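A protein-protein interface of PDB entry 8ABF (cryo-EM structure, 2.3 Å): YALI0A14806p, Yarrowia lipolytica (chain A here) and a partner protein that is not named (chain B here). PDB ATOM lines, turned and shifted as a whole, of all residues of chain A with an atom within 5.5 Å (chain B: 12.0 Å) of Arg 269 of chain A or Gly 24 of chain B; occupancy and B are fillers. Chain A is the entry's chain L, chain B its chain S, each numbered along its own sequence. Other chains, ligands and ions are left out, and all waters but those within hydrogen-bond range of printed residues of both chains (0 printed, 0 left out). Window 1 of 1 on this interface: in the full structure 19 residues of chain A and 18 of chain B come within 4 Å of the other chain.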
ATOM      1  N   GLU A 267      -9.353 -11.119   6.642  1.00  0.00           N
ATOM      2  CA  GLU A 267     -10.766 -11.106   6.309  1.00  0.00           C
ATOM      3  C   GLU A 267     -11.412  -9.835   6.822  1.00  0.00           C
ATOM      4  O   GLU A 267     -10.973  -9.279   7.826  1.00  0.00           O
ATOM      5  CB  GLU A 267     -11.536 -12.324   6.810  1.00  0.00           C
ATOM      6  CG  GLU A 267     -11.079 -12.754   8.164  1.00  0.00           C
ATOM      7  CD  GLU A 267     -12.017 -13.751   8.819  1.00  0.00           C
ATOM      8  OE1 GLU A 267     -12.312 -14.813   8.209  1.00  0.00           O
ATOM      9  OE2 GLU A 267     -12.441 -13.490   9.959  1.00  0.00           O
ATOM     10  N   VAL A 268     -12.443  -9.405   6.094  1.00  0.00           N
ATOM     11  CA  VAL A 268     -13.324  -8.357   6.558  1.00  0.00           C
ATOM     12  C   VAL A 268     -14.716  -8.960   6.569  1.00  0.00           C
ATOM     13  O   VAL A 268     -15.142  -9.505   5.561  1.00  0.00           O
ATOM     14  CB  VAL A 268     -13.286  -7.116   5.647  1.00  0.00           C
ATOM     15  CG1 VAL A 268     -14.196  -6.018   6.183  1.00  0.00           C
ATOM     16  CG2 VAL A 268     -11.875  -6.584   5.460  1.00  0.00           C
ATOM     17  N   ARG A 269     -15.418  -8.852   7.696  1.00  0.00           N
ATOM     18  CA  ARG A 269     -16.792  -9.322   7.746  1.00  0.00           C
ATOM     19  C   ARG A 269     -17.705  -8.135   7.977  1.00  0.00           C
ATOM     20  O   ARG A 269     -17.495  -7.385   8.924  1.00  0.00           O
ATOM     21  CB  ARG A 269     -16.993 -10.301   8.894  1.00  0.00           C
ATOM     22  CG  ARG A 269     -16.246 -11.599   8.670  1.00  0.00           C
ATOM     23  CD  ARG A 269     -16.030 -12.394   9.930  1.00  0.00           C
ATOM     24  NE  ARG A 269     -16.733 -13.579   9.518  1.00  0.00           N
ATOM     25  CZ  ARG A 269     -16.211 -14.719   9.099  1.00  0.00           C
ATOM     26  NH1 ARG A 269     -14.914 -14.979   9.112  1.00  0.00           N
ATOM     27  NH2 ARG A 269     -17.065 -15.644   8.726  1.00  0.00           N
ATOM     28  N   LEU A 270     -18.682  -7.955   7.091  1.00  0.00           N
ATOM     29  CA  LEU A 270     -19.583  -6.826   7.210  1.00  0.00           C
ATOM     30  C   LEU A 270     -20.969  -7.421   7.346  1.00  0.00           C
ATOM     31  O   LEU A 270     -21.731  -7.475   6.389  1.00  0.00           O
ATOM     32  CB  LEU A 270     -19.453  -5.955   5.956  1.00  0.00           C
ATOM     33  CG  LEU A 270     -18.052  -5.426   5.649  1.00  0.00           C
ATOM     34  CD1 LEU A 270     -17.966  -4.900   4.222  1.00  0.00           C
ATOM     35  CD2 LEU A 270     -17.644  -4.336   6.630  1.00  0.00           C
ATOM     36  N   ARG A 271     -21.240  -7.982   8.515  1.00  0.00           N
ATOM     37  CA  ARG A 271     -22.470  -8.733   8.615  1.00  0.00           C
ATOM     38  C   ARG A 271     -23.632  -7.752   8.653  1.00  0.00           C
ATOM     39  O   ARG A 271     -23.553  -6.734   9.329  1.00  0.00           O
ATOM     40  CB  ARG A 271     -22.445  -9.572   9.883  1.00  0.00           C
ATOM     41  CG  ARG A 271     -23.772 -10.240  10.181  1.00  0.00           C
ATOM     42  CD  ARG A 271     -23.450 -11.365  11.133  1.00  0.00           C
ATOM     43  NE  ARG A 271     -24.698 -11.865  11.676  1.00  0.00           N
ATOM     44  CZ  ARG A 271     -24.808 -12.800  12.611  1.00  0.00           C
ATOM     45  NH1 ARG A 271     -23.731 -13.357  13.143  1.00  0.00           N
ATOM     46  NH2 ARG A 271     -26.012 -13.158  13.019  1.00  0.00           N
ATOM     47  N   LEU A 450     -10.503 -12.480   2.291  1.00  0.00           N
ATOM     48  CA  LEU A 450     -11.889 -12.893   2.254  1.00  0.00           C
ATOM     49  C   LEU A 450     -12.740 -11.712   2.703  1.00  0.00           C
ATOM     50  O   LEU A 450     -12.423 -11.074   3.700  1.00  0.00           O
ATOM     51  CB  LEU A 450     -11.965 -14.061   3.235  1.00  0.00           C
ATOM     52  CG  LEU A 450     -13.345 -14.388   3.793  1.00  0.00           C
ATOM     53  CD1 LEU A 450     -14.168 -15.124   2.758  1.00  0.00           C
ATOM     54  CD2 LEU A 450     -13.206 -15.274   5.021  1.00  0.00           C
ATOM     55  N   GLY A 452     -16.883 -10.700   3.415  1.00  0.00           N
ATOM     56  CA  GLY A 452     -18.249 -11.166   3.406  1.00  0.00           C
ATOM     57  C   GLY A 452     -19.157 -10.004   3.758  1.00  0.00           C
ATOM     58  O   GLY A 452     -18.867  -9.274   4.691  1.00  0.00           O
ATOM     59  N   ILE A 456     -24.134 -13.288   6.845  1.00  0.00           N
ATOM     60  CA  ILE A 456     -22.995 -14.178   6.677  1.00  0.00           C
ATOM     61  C   ILE A 456     -22.708 -14.938   7.969  1.00  0.00           C
ATOM     62  O   ILE A 456     -21.605 -15.437   8.159  1.00  0.00           O
ATOM     63  CB  ILE A 456     -21.766 -13.385   6.203  1.00  0.00           C
ATOM     64  CG1 ILE A 456     -21.490 -12.244   7.191  1.00  0.00           C
ATOM     65  CG2 ILE A 456     -21.960 -12.903   4.765  1.00  0.00           C
ATOM     66  CD1 ILE A 456     -20.125 -11.583   7.067  1.00  0.00           C
ATOM     67  N   LEU A 459     -20.991 -18.062   7.431  1.00  0.00           N
ATOM     68  CA  LEU A 459     -19.665 -18.138   6.843  1.00  0.00           C
ATOM     69  C   LEU A 459     -18.735 -18.487   7.996  1.00  0.00           C
ATOM     70  O   LEU A 459     -18.761 -17.773   8.979  1.00  0.00           O
ATOM     71  CB  LEU A 459     -19.348 -16.762   6.248  1.00  0.00           C
ATOM     72  CG  LEU A 459     -17.942 -16.588   5.684  1.00  0.00           C
ATOM     73  CD1 LEU A 459     -17.736 -17.490   4.483  1.00  0.00           C
ATOM     74  CD2 LEU A 459     -17.680 -15.136   5.305  1.00  0.00           C
ATOM     75  N   TYR A 460     -17.995 -19.603   7.945  1.00  0.00           N
ATOM     76  CA  TYR A 460     -17.185 -19.967   9.103  1.00  0.00           C
ATOM     77  C   TYR A 460     -16.011 -19.010   9.276  1.00  0.00           C
ATOM     78  O   TYR A 460     -15.746 -18.201   8.398  1.00  0.00           O
ATOM     79  CB  TYR A 460     -16.618 -21.379   8.973  1.00  0.00           C
ATOM     80  CG  TYR A 460     -17.663 -22.465   9.035  1.00  0.00           C
ATOM     81  CD1 TYR A 460     -18.706 -22.397   9.950  1.00  0.00           C
ATOM     82  CD2 TYR A 460     -17.619 -23.557   8.177  1.00  0.00           C
ATOM     83  CE1 TYR A 460     -19.684 -23.379  10.002  1.00  0.00           C
ATOM     84  CE2 TYR A 460     -18.579 -24.562   8.231  1.00  0.00           C
ATOM     85  CZ  TYR A 460     -19.626 -24.459   9.134  1.00  0.00           C
ATOM     86  OH  TYR A 460     -20.563 -25.447   9.206  1.00  0.00           O
ATOM     87  N   ASP A 461     -15.302 -19.139  10.393  1.00  0.00           N
ATOM     88  CA  ASP A 461     -14.140 -18.323  10.708  1.00  0.00           C
ATOM     89  C   ASP A 461     -13.011 -18.543   9.695  1.00  0.00           C
ATOM     90  O   ASP A 461     -13.024 -19.503   8.917  1.00  0.00           O
ATOM     91  CB  ASP A 461     -13.710 -18.671  12.131  1.00  0.00           C
ATOM     92  CG  ASP A 461     -13.693 -20.175  12.344  1.00  0.00           C
ATOM     93  OD1 ASP A 461     -12.873 -20.827  11.684  1.00  0.00           O
ATOM     94  OD2 ASP A 461     -14.511 -20.687  13.159  1.00  0.00           O
ATOM     95  N   TYR A 462     -12.006 -17.659   9.738  1.00  0.00           N
ATOM     96  CA  TYR A 462     -10.913 -17.689   8.783  1.00  0.00           C
ATOM     97  C   TYR A 462     -10.274 -19.077   8.671  1.00  0.00           C
ATOM     98  O   TYR A 462     -10.052 -19.526   7.557  1.00  0.00           O
ATOM     99  CB  TYR A 462      -9.895 -16.584   9.061  1.00  0.00           C
ATOM    100  CG  TYR A 462      -8.861 -16.447   7.970  1.00  0.00           C
ATOM    101  CD1 TYR A 462      -7.703 -17.226   7.968  1.00  0.00           C
ATOM    102  CD2 TYR A 462      -9.019 -15.536   6.929  1.00  0.00           C
ATOM    103  CE1 TYR A 462      -6.749 -17.118   6.961  1.00  0.00           C
ATOM    104  CE2 TYR A 462      -8.072 -15.419   5.913  1.00  0.00           C
ATOM    105  CZ  TYR A 462      -6.926 -16.204   5.930  1.00  0.00           C
ATOM    106  OH  TYR A 462      -5.991 -16.094   4.926  1.00  0.00           O
ATOM    107  N   TRP B  11     -25.832 -22.760  12.539  1.00  0.00           N
ATOM    108  CA  TRP B  11     -25.217 -21.764  11.672  1.00  0.00           C
ATOM    109  C   TRP B  11     -26.206 -21.208  10.654  1.00  0.00           C
ATOM    110  O   TRP B  11     -26.856 -21.969   9.941  1.00  0.00           O
ATOM    111  CB  TRP B  11     -24.045 -22.407  10.950  1.00  0.00           C
ATOM    112  CG  TRP B  11     -23.020 -22.897  11.913  1.00  0.00           C
ATOM    113  CD1 TRP B  11     -22.788 -24.188  12.288  1.00  0.00           C
ATOM    114  CD2 TRP B  11     -22.081 -22.083  12.638  1.00  0.00           C
ATOM    115  NE1 TRP B  11     -21.748 -24.232  13.180  1.00  0.00           N
ATOM    116  CE2 TRP B  11     -21.297 -22.959  13.418  1.00  0.00           C
ATOM    117  CE3 TRP B  11     -21.825 -20.702  12.704  1.00  0.00           C
ATOM    118  CZ2 TRP B  11     -20.269 -22.496  14.247  1.00  0.00           C
ATOM    119  CZ3 TRP B  11     -20.813 -20.244  13.525  1.00  0.00           C
ATOM    120  CH2 TRP B  11     -20.045 -21.134  14.286  1.00  0.00           C
ATOM    121  N   GLY B  12     -26.295 -19.875  10.574  1.00  0.00           N
ATOM    122  CA  GLY B  12     -27.211 -19.244   9.645  1.00  0.00           C
ATOM    123  C   GLY B  12     -28.508 -18.832  10.332  1.00  0.00           C
ATOM    124  O   GLY B  12     -29.202 -17.957   9.834  1.00  0.00           O
ATOM    125  N   MET B  14     -28.663 -18.720  14.192  1.00  0.00           N
ATOM    126  CA  MET B  14     -28.183 -19.094  15.508  1.00  0.00           C
ATOM    127  C   MET B  14     -29.142 -18.611  16.601  1.00  0.00           C
ATOM    128  O   MET B  14     -29.131 -19.166  17.688  1.00  0.00           O
ATOM    129  CB  MET B  14     -26.782 -18.539  15.774  1.00  0.00           C
ATOM    130  CG  MET B  14     -26.059 -19.224  16.929  1.00  0.00           C
ATOM    131  SD  MET B  14     -25.648 -20.961  16.583  1.00  0.00           S
ATOM    132  CE  MET B  14     -24.530 -20.744  15.194  1.00  0.00           C
ATOM    133  N   GLN B  19     -27.921  -8.401  13.468  1.00  0.00           N
ATOM    134  CA  GLN B  19     -26.681  -7.678  13.623  1.00  0.00           C
ATOM    135  C   GLN B  19     -26.550  -6.746  12.433  1.00  0.00           C
ATOM    136  O   GLN B  19     -26.851  -7.128  11.302  1.00  0.00           O
ATOM    137  CB  GLN B  19     -25.516  -8.655  13.681  1.00  0.00           C
ATOM    138  CG  GLN B  19     -25.685  -9.710  14.760  1.00  0.00           C
ATOM    139  CD  GLN B  19     -24.379 -10.402  15.070  1.00  0.00           C
ATOM    140  OE1 GLN B  19     -23.325 -10.042  14.548  1.00  0.00           O
ATOM    141  NE2 GLN B  19     -24.435 -11.408  15.930  1.00  0.00           N
ATOM    142  N   LYS B  20     -26.124  -5.520  12.713  1.00  0.00           N
ATOM    143  CA  LYS B  20     -25.848  -4.576  11.653  1.00  0.00           C
ATOM    144  C   LYS B  20     -24.846  -3.553  12.162  1.00  0.00           C
ATOM    145  O   LYS B  20     -24.893  -3.193  13.323  1.00  0.00           O
ATOM    146  CB  LYS B  20     -27.131  -3.839  11.293  1.00  0.00           C
ATOM    147  CG  LYS B  20     -27.034  -3.154   9.958  1.00  0.00           C
ATOM    148  CD  LYS B  20     -28.364  -2.592   9.541  1.00  0.00           C
ATOM    149  CE  LYS B  20     -28.259  -1.657   8.358  1.00  0.00           C
ATOM    150  NZ  LYS B  20     -29.599  -1.317   7.822  1.00  0.00           N
ATOM    151  N   GLY B  21     -23.952  -3.085  11.287  1.00  0.00           N
ATOM    152  CA  GLY B  21     -23.103  -1.958  11.625  1.00  0.00           C
ATOM    153  C   GLY B  21     -21.757  -2.351  12.228  1.00  0.00           C
ATOM    154  O   GLY B  21     -20.936  -1.471  12.473  1.00  0.00           O
ATOM    155  N   ILE B  22     -21.498  -3.645  12.437  1.00  0.00           N
ATOM    156  CA  ILE B  22     -20.209  -4.044  12.989  1.00  0.00           C
ATOM    157  C   ILE B  22     -19.321  -4.560  11.867  1.00  0.00           C
ATOM    158  O   ILE B  22     -19.703  -5.489  11.172  1.00  0.00           O
ATOM    159  CB  ILE B  22     -20.385  -5.132  14.062  1.00  0.00           C
ATOM    160  CG1 ILE B  22     -21.388  -4.699  15.132  1.00  0.00           C
ATOM    161  CG2 ILE B  22     -19.037  -5.531  14.651  1.00  0.00           C
ATOM    162  CD1 ILE B  22     -21.920  -5.842  15.972  1.00  0.00           C
ATOM    163  N   ALA B  23     -18.124  -3.997  11.716  1.00  0.00           N
ATOM    164  CA  ALA B  23     -17.193  -4.564  10.763  1.00  0.00           C
ATOM    165  C   ALA B  23     -16.148  -5.310  11.578  1.00  0.00           C
ATOM    166  O   ALA B  23     -15.651  -4.747  12.545  1.00  0.00           O
ATOM    167  CB  ALA B  23     -16.591  -3.452   9.952  1.00  0.00           C
ATOM    168  N   GLY B  24     -15.856  -6.564  11.218  1.00  0.00           N
ATOM    169  CA  GLY B  24     -14.877  -7.357  11.942  1.00  0.00           C
ATOM    170  C   GLY B  24     -13.672  -7.629  11.051  1.00  0.00           C
ATOM    171  O   GLY B  24     -13.833  -7.853   9.859  1.00  0.00           O
ATOM    172  N   TYR B  25     -12.475  -7.581  11.628  1.00  0.00           N
ATOM    173  CA  TYR B  25     -11.273  -7.728  10.832  1.00  0.00           C
ATOM    174  C   TYR B  25     -10.350  -8.708  11.524  1.00  0.00           C
ATOM    175  O   TYR B  25     -10.249  -8.692  12.745  1.00  0.00           O
ATOM    176  CB  TYR B  25     -10.536  -6.393  10.779  1.00  0.00           C
ATOM    177  CG  TYR B  25     -11.355  -5.277  10.187  1.00  0.00           C
ATOM    178  CD1 TYR B  25     -12.268  -4.566  10.961  1.00  0.00           C
ATOM    179  CD2 TYR B  25     -11.221  -4.935   8.848  1.00  0.00           C
ATOM    180  CE1 TYR B  25     -13.018  -3.533  10.426  1.00  0.00           C
ATOM    181  CE2 TYR B  25     -11.968  -3.909   8.289  1.00  0.00           C
ATOM    182  CZ  TYR B  25     -12.856  -3.208   9.090  1.00  0.00           C
ATOM    183  OH  TYR B  25     -13.594  -2.205   8.563  1.00  0.00           O
ATOM    184  N   THR B  26      -9.652  -9.538  10.757  1.00  0.00           N
ATOM    185  CA  THR B  26      -8.582 -10.302  11.376  1.00  0.00           C
ATOM    186  C   THR B  26      -7.582 -10.722  10.316  1.00  0.00           C
ATOM    187  O   THR B  26      -7.840 -10.539   9.141  1.00  0.00           O
ATOM    188  CB  THR B  26      -9.101 -11.509  12.167  1.00  0.00           C
ATOM    189  OG1 THR B  26      -7.990 -11.954  12.946  1.00  0.00           O
ATOM    190  CG2 THR B  26      -9.611 -12.636  11.297  1.00  0.00           C
ATOM    191  N   ILE B  27      -6.471 -11.335  10.731  1.00  0.00           N
ATOM    192  CA  ILE B  27      -5.425 -11.704   9.792  1.00  0.00           C
ATOM    193  C   ILE B  27      -5.145 -13.194   9.931  1.00  0.00           C
ATOM    194  O   ILE B  27      -5.426 -13.791  10.963  1.00  0.00           O
ATOM    195  CB  ILE B  27      -4.164 -10.849  10.025  1.00  0.00           C
ATOM    196  CG1 ILE B  27      -3.651 -10.995  11.462  1.00  0.00           C
ATOM    197  CG2 ILE B  27      -4.416  -9.390   9.656  1.00  0.00           C
ATOM    198  CD1 ILE B  27      -2.253 -10.446  11.687  1.00  0.00           C
ATOM    199  N   SER B  28      -4.527 -13.759   8.901  1.00  0.00           N
ATOM    200  CA  SER B  28      -4.254 -15.180   8.806  1.00  0.00           C
ATOM    201  C   SER B  28      -3.348 -15.664   9.941  1.00  0.00           C
ATOM    202  O   SER B  28      -2.485 -14.926  10.409  1.00  0.00           O
ATOM    203  CB  SER B  28      -3.608 -15.404   7.487  1.00  0.00           C
ATOM    204  OG  SER B  28      -3.098 -16.714   7.396  1.00  0.00           O
ATOM    205  N   PRO B  29      -3.464 -16.929  10.408  1.00  0.00           N
ATOM    206  CA  PRO B  29      -2.536 -17.433  11.416  1.00  0.00           C
ATOM    207  C   PRO B  29      -1.108 -17.469  10.881  1.00  0.00           C
ATOM    208  O   PRO B  29      -0.175 -17.244  11.644  1.00  0.00           O
ATOM    209  CB  PRO B  29      -3.080 -18.819  11.762  1.00  0.00           C
ATOM    210  CG  PRO B  29      -3.863 -19.222  10.540  1.00  0.00           C
ATOM    211  CD  PRO B  29      -4.466 -17.935  10.019  1.00  0.00           C
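The backbone NH (N) of Arg 269 of chain A sits at hydrogen-bond distance from the backbone carbonyl oxygen (O) of Gly 24 of chain B (2.9 Å). The backbone NH (N) of Glu 267 of chain A lies within hydrogen-bond range of the backbone carbonyl oxygen (O) of Thr 26 of chain B (3.0 Å). NE2 of Gln 19 of chain B lies close to NH1 of Arg 271 of chain A (3.5 Å).
NH2 of Arg 269 of chain A is in hydrogen-bond range of O of Tyr 460 of chain A (2.9 Å). OE1 of Glu 267 of chain A lies close to N of Tyr 462 of chain A (3.2 Å). O of Gly 452 of chain A lies within hydrogen-bond range of N of Leu 270 of chain A, at 2.7 Å. NH2 of Arg 269 of chain A sits at hydrogen-bond distance from O of Leu 459 of chain A (2.7 Å). The backbone NH (N) of Val 268 of chain A is in hydrogen-bond range of the backbone carbonyl oxygen (O) of Leu 450 of chain A. The side-chain carboxylate (OE1) of Glu 267 of chain A is in salt-bridge range of the guanidinium group (NH1) of Arg 269 of chain A, 2.8 Å away.
O of Glu 267 of chain A touches O of Gly 24 of chain B (3.8 Å). Glu 267 of chain A touches Tyr 25 of chain B (O to CA, 3.4 Å). Val 268 of chain A touches Tyr 25 of chain B (CG1 to CE2, 3.7 Å). Arg 269 of chain A touches Ile 22 of chain B. O of Arg 269 of chain A touches CA of Ala 23 of chain B, at 3.4 Å. Ala 23 of chain B touches Leu 270 of chain A (CB to CD2, 3.6 Å). O of Arg 271 of chain A touches CA of Lys 20 of chain B, 3.9 Å away. Ile 22 of chain B touches Arg 271 of chain A (O to N, 3.95 Å). Trp 11 of chain B touches Tyr 460 of chain A. Ser 28 of chain B touches Tyr 462 of chain A (CB to OH, 3.6 Å).
Arg 269 of chain A touches three residues of chain B. Glu 267 of chain A touches three residues of chain B. Val 268 of chain A touches two residues of chain B. No residue of chain B comes within 4 Å of Gly 452 of chain A. No residue of chain B comes within 4 Å of Ile 456 of chain A. No residue of chain B comes within 4 Å of Leu 459 of chain A. Of the printed residues of chain A, Ala 23 of chain B touches Arg 269 and Leu 270. Printed residues of chain A within 4 Å of Gln 19 of chain B: Arg 271. Of the printed residues of chain B, Tyr 460 of chain A touches Trp 11 (3.8 Å). Of the printed residues of chain A, Tyr 25 of chain B touches Glu 267 and Val 268. Leu 450 of chain A touches none of the printed residues of chain B. Gly 12 of chain B touches none of the printed residues of chain A. The nearest residue of chain B that does not touch Arg 269 of chain A is Tyr 25 of chain B (5.1 Å).
Along chain B the printed residues that touch a printed residue of chain A span positions 11 to 29. Of the 12 printed residues of chain A, 7 touch a printed residue of chain B. Among the printed residues, 15 pairs touch across the chains. Among the printed residues, no Asp or Glu carboxylate lies within 4 Å of a Lys or Arg side-chain nitrogen of the other chain.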
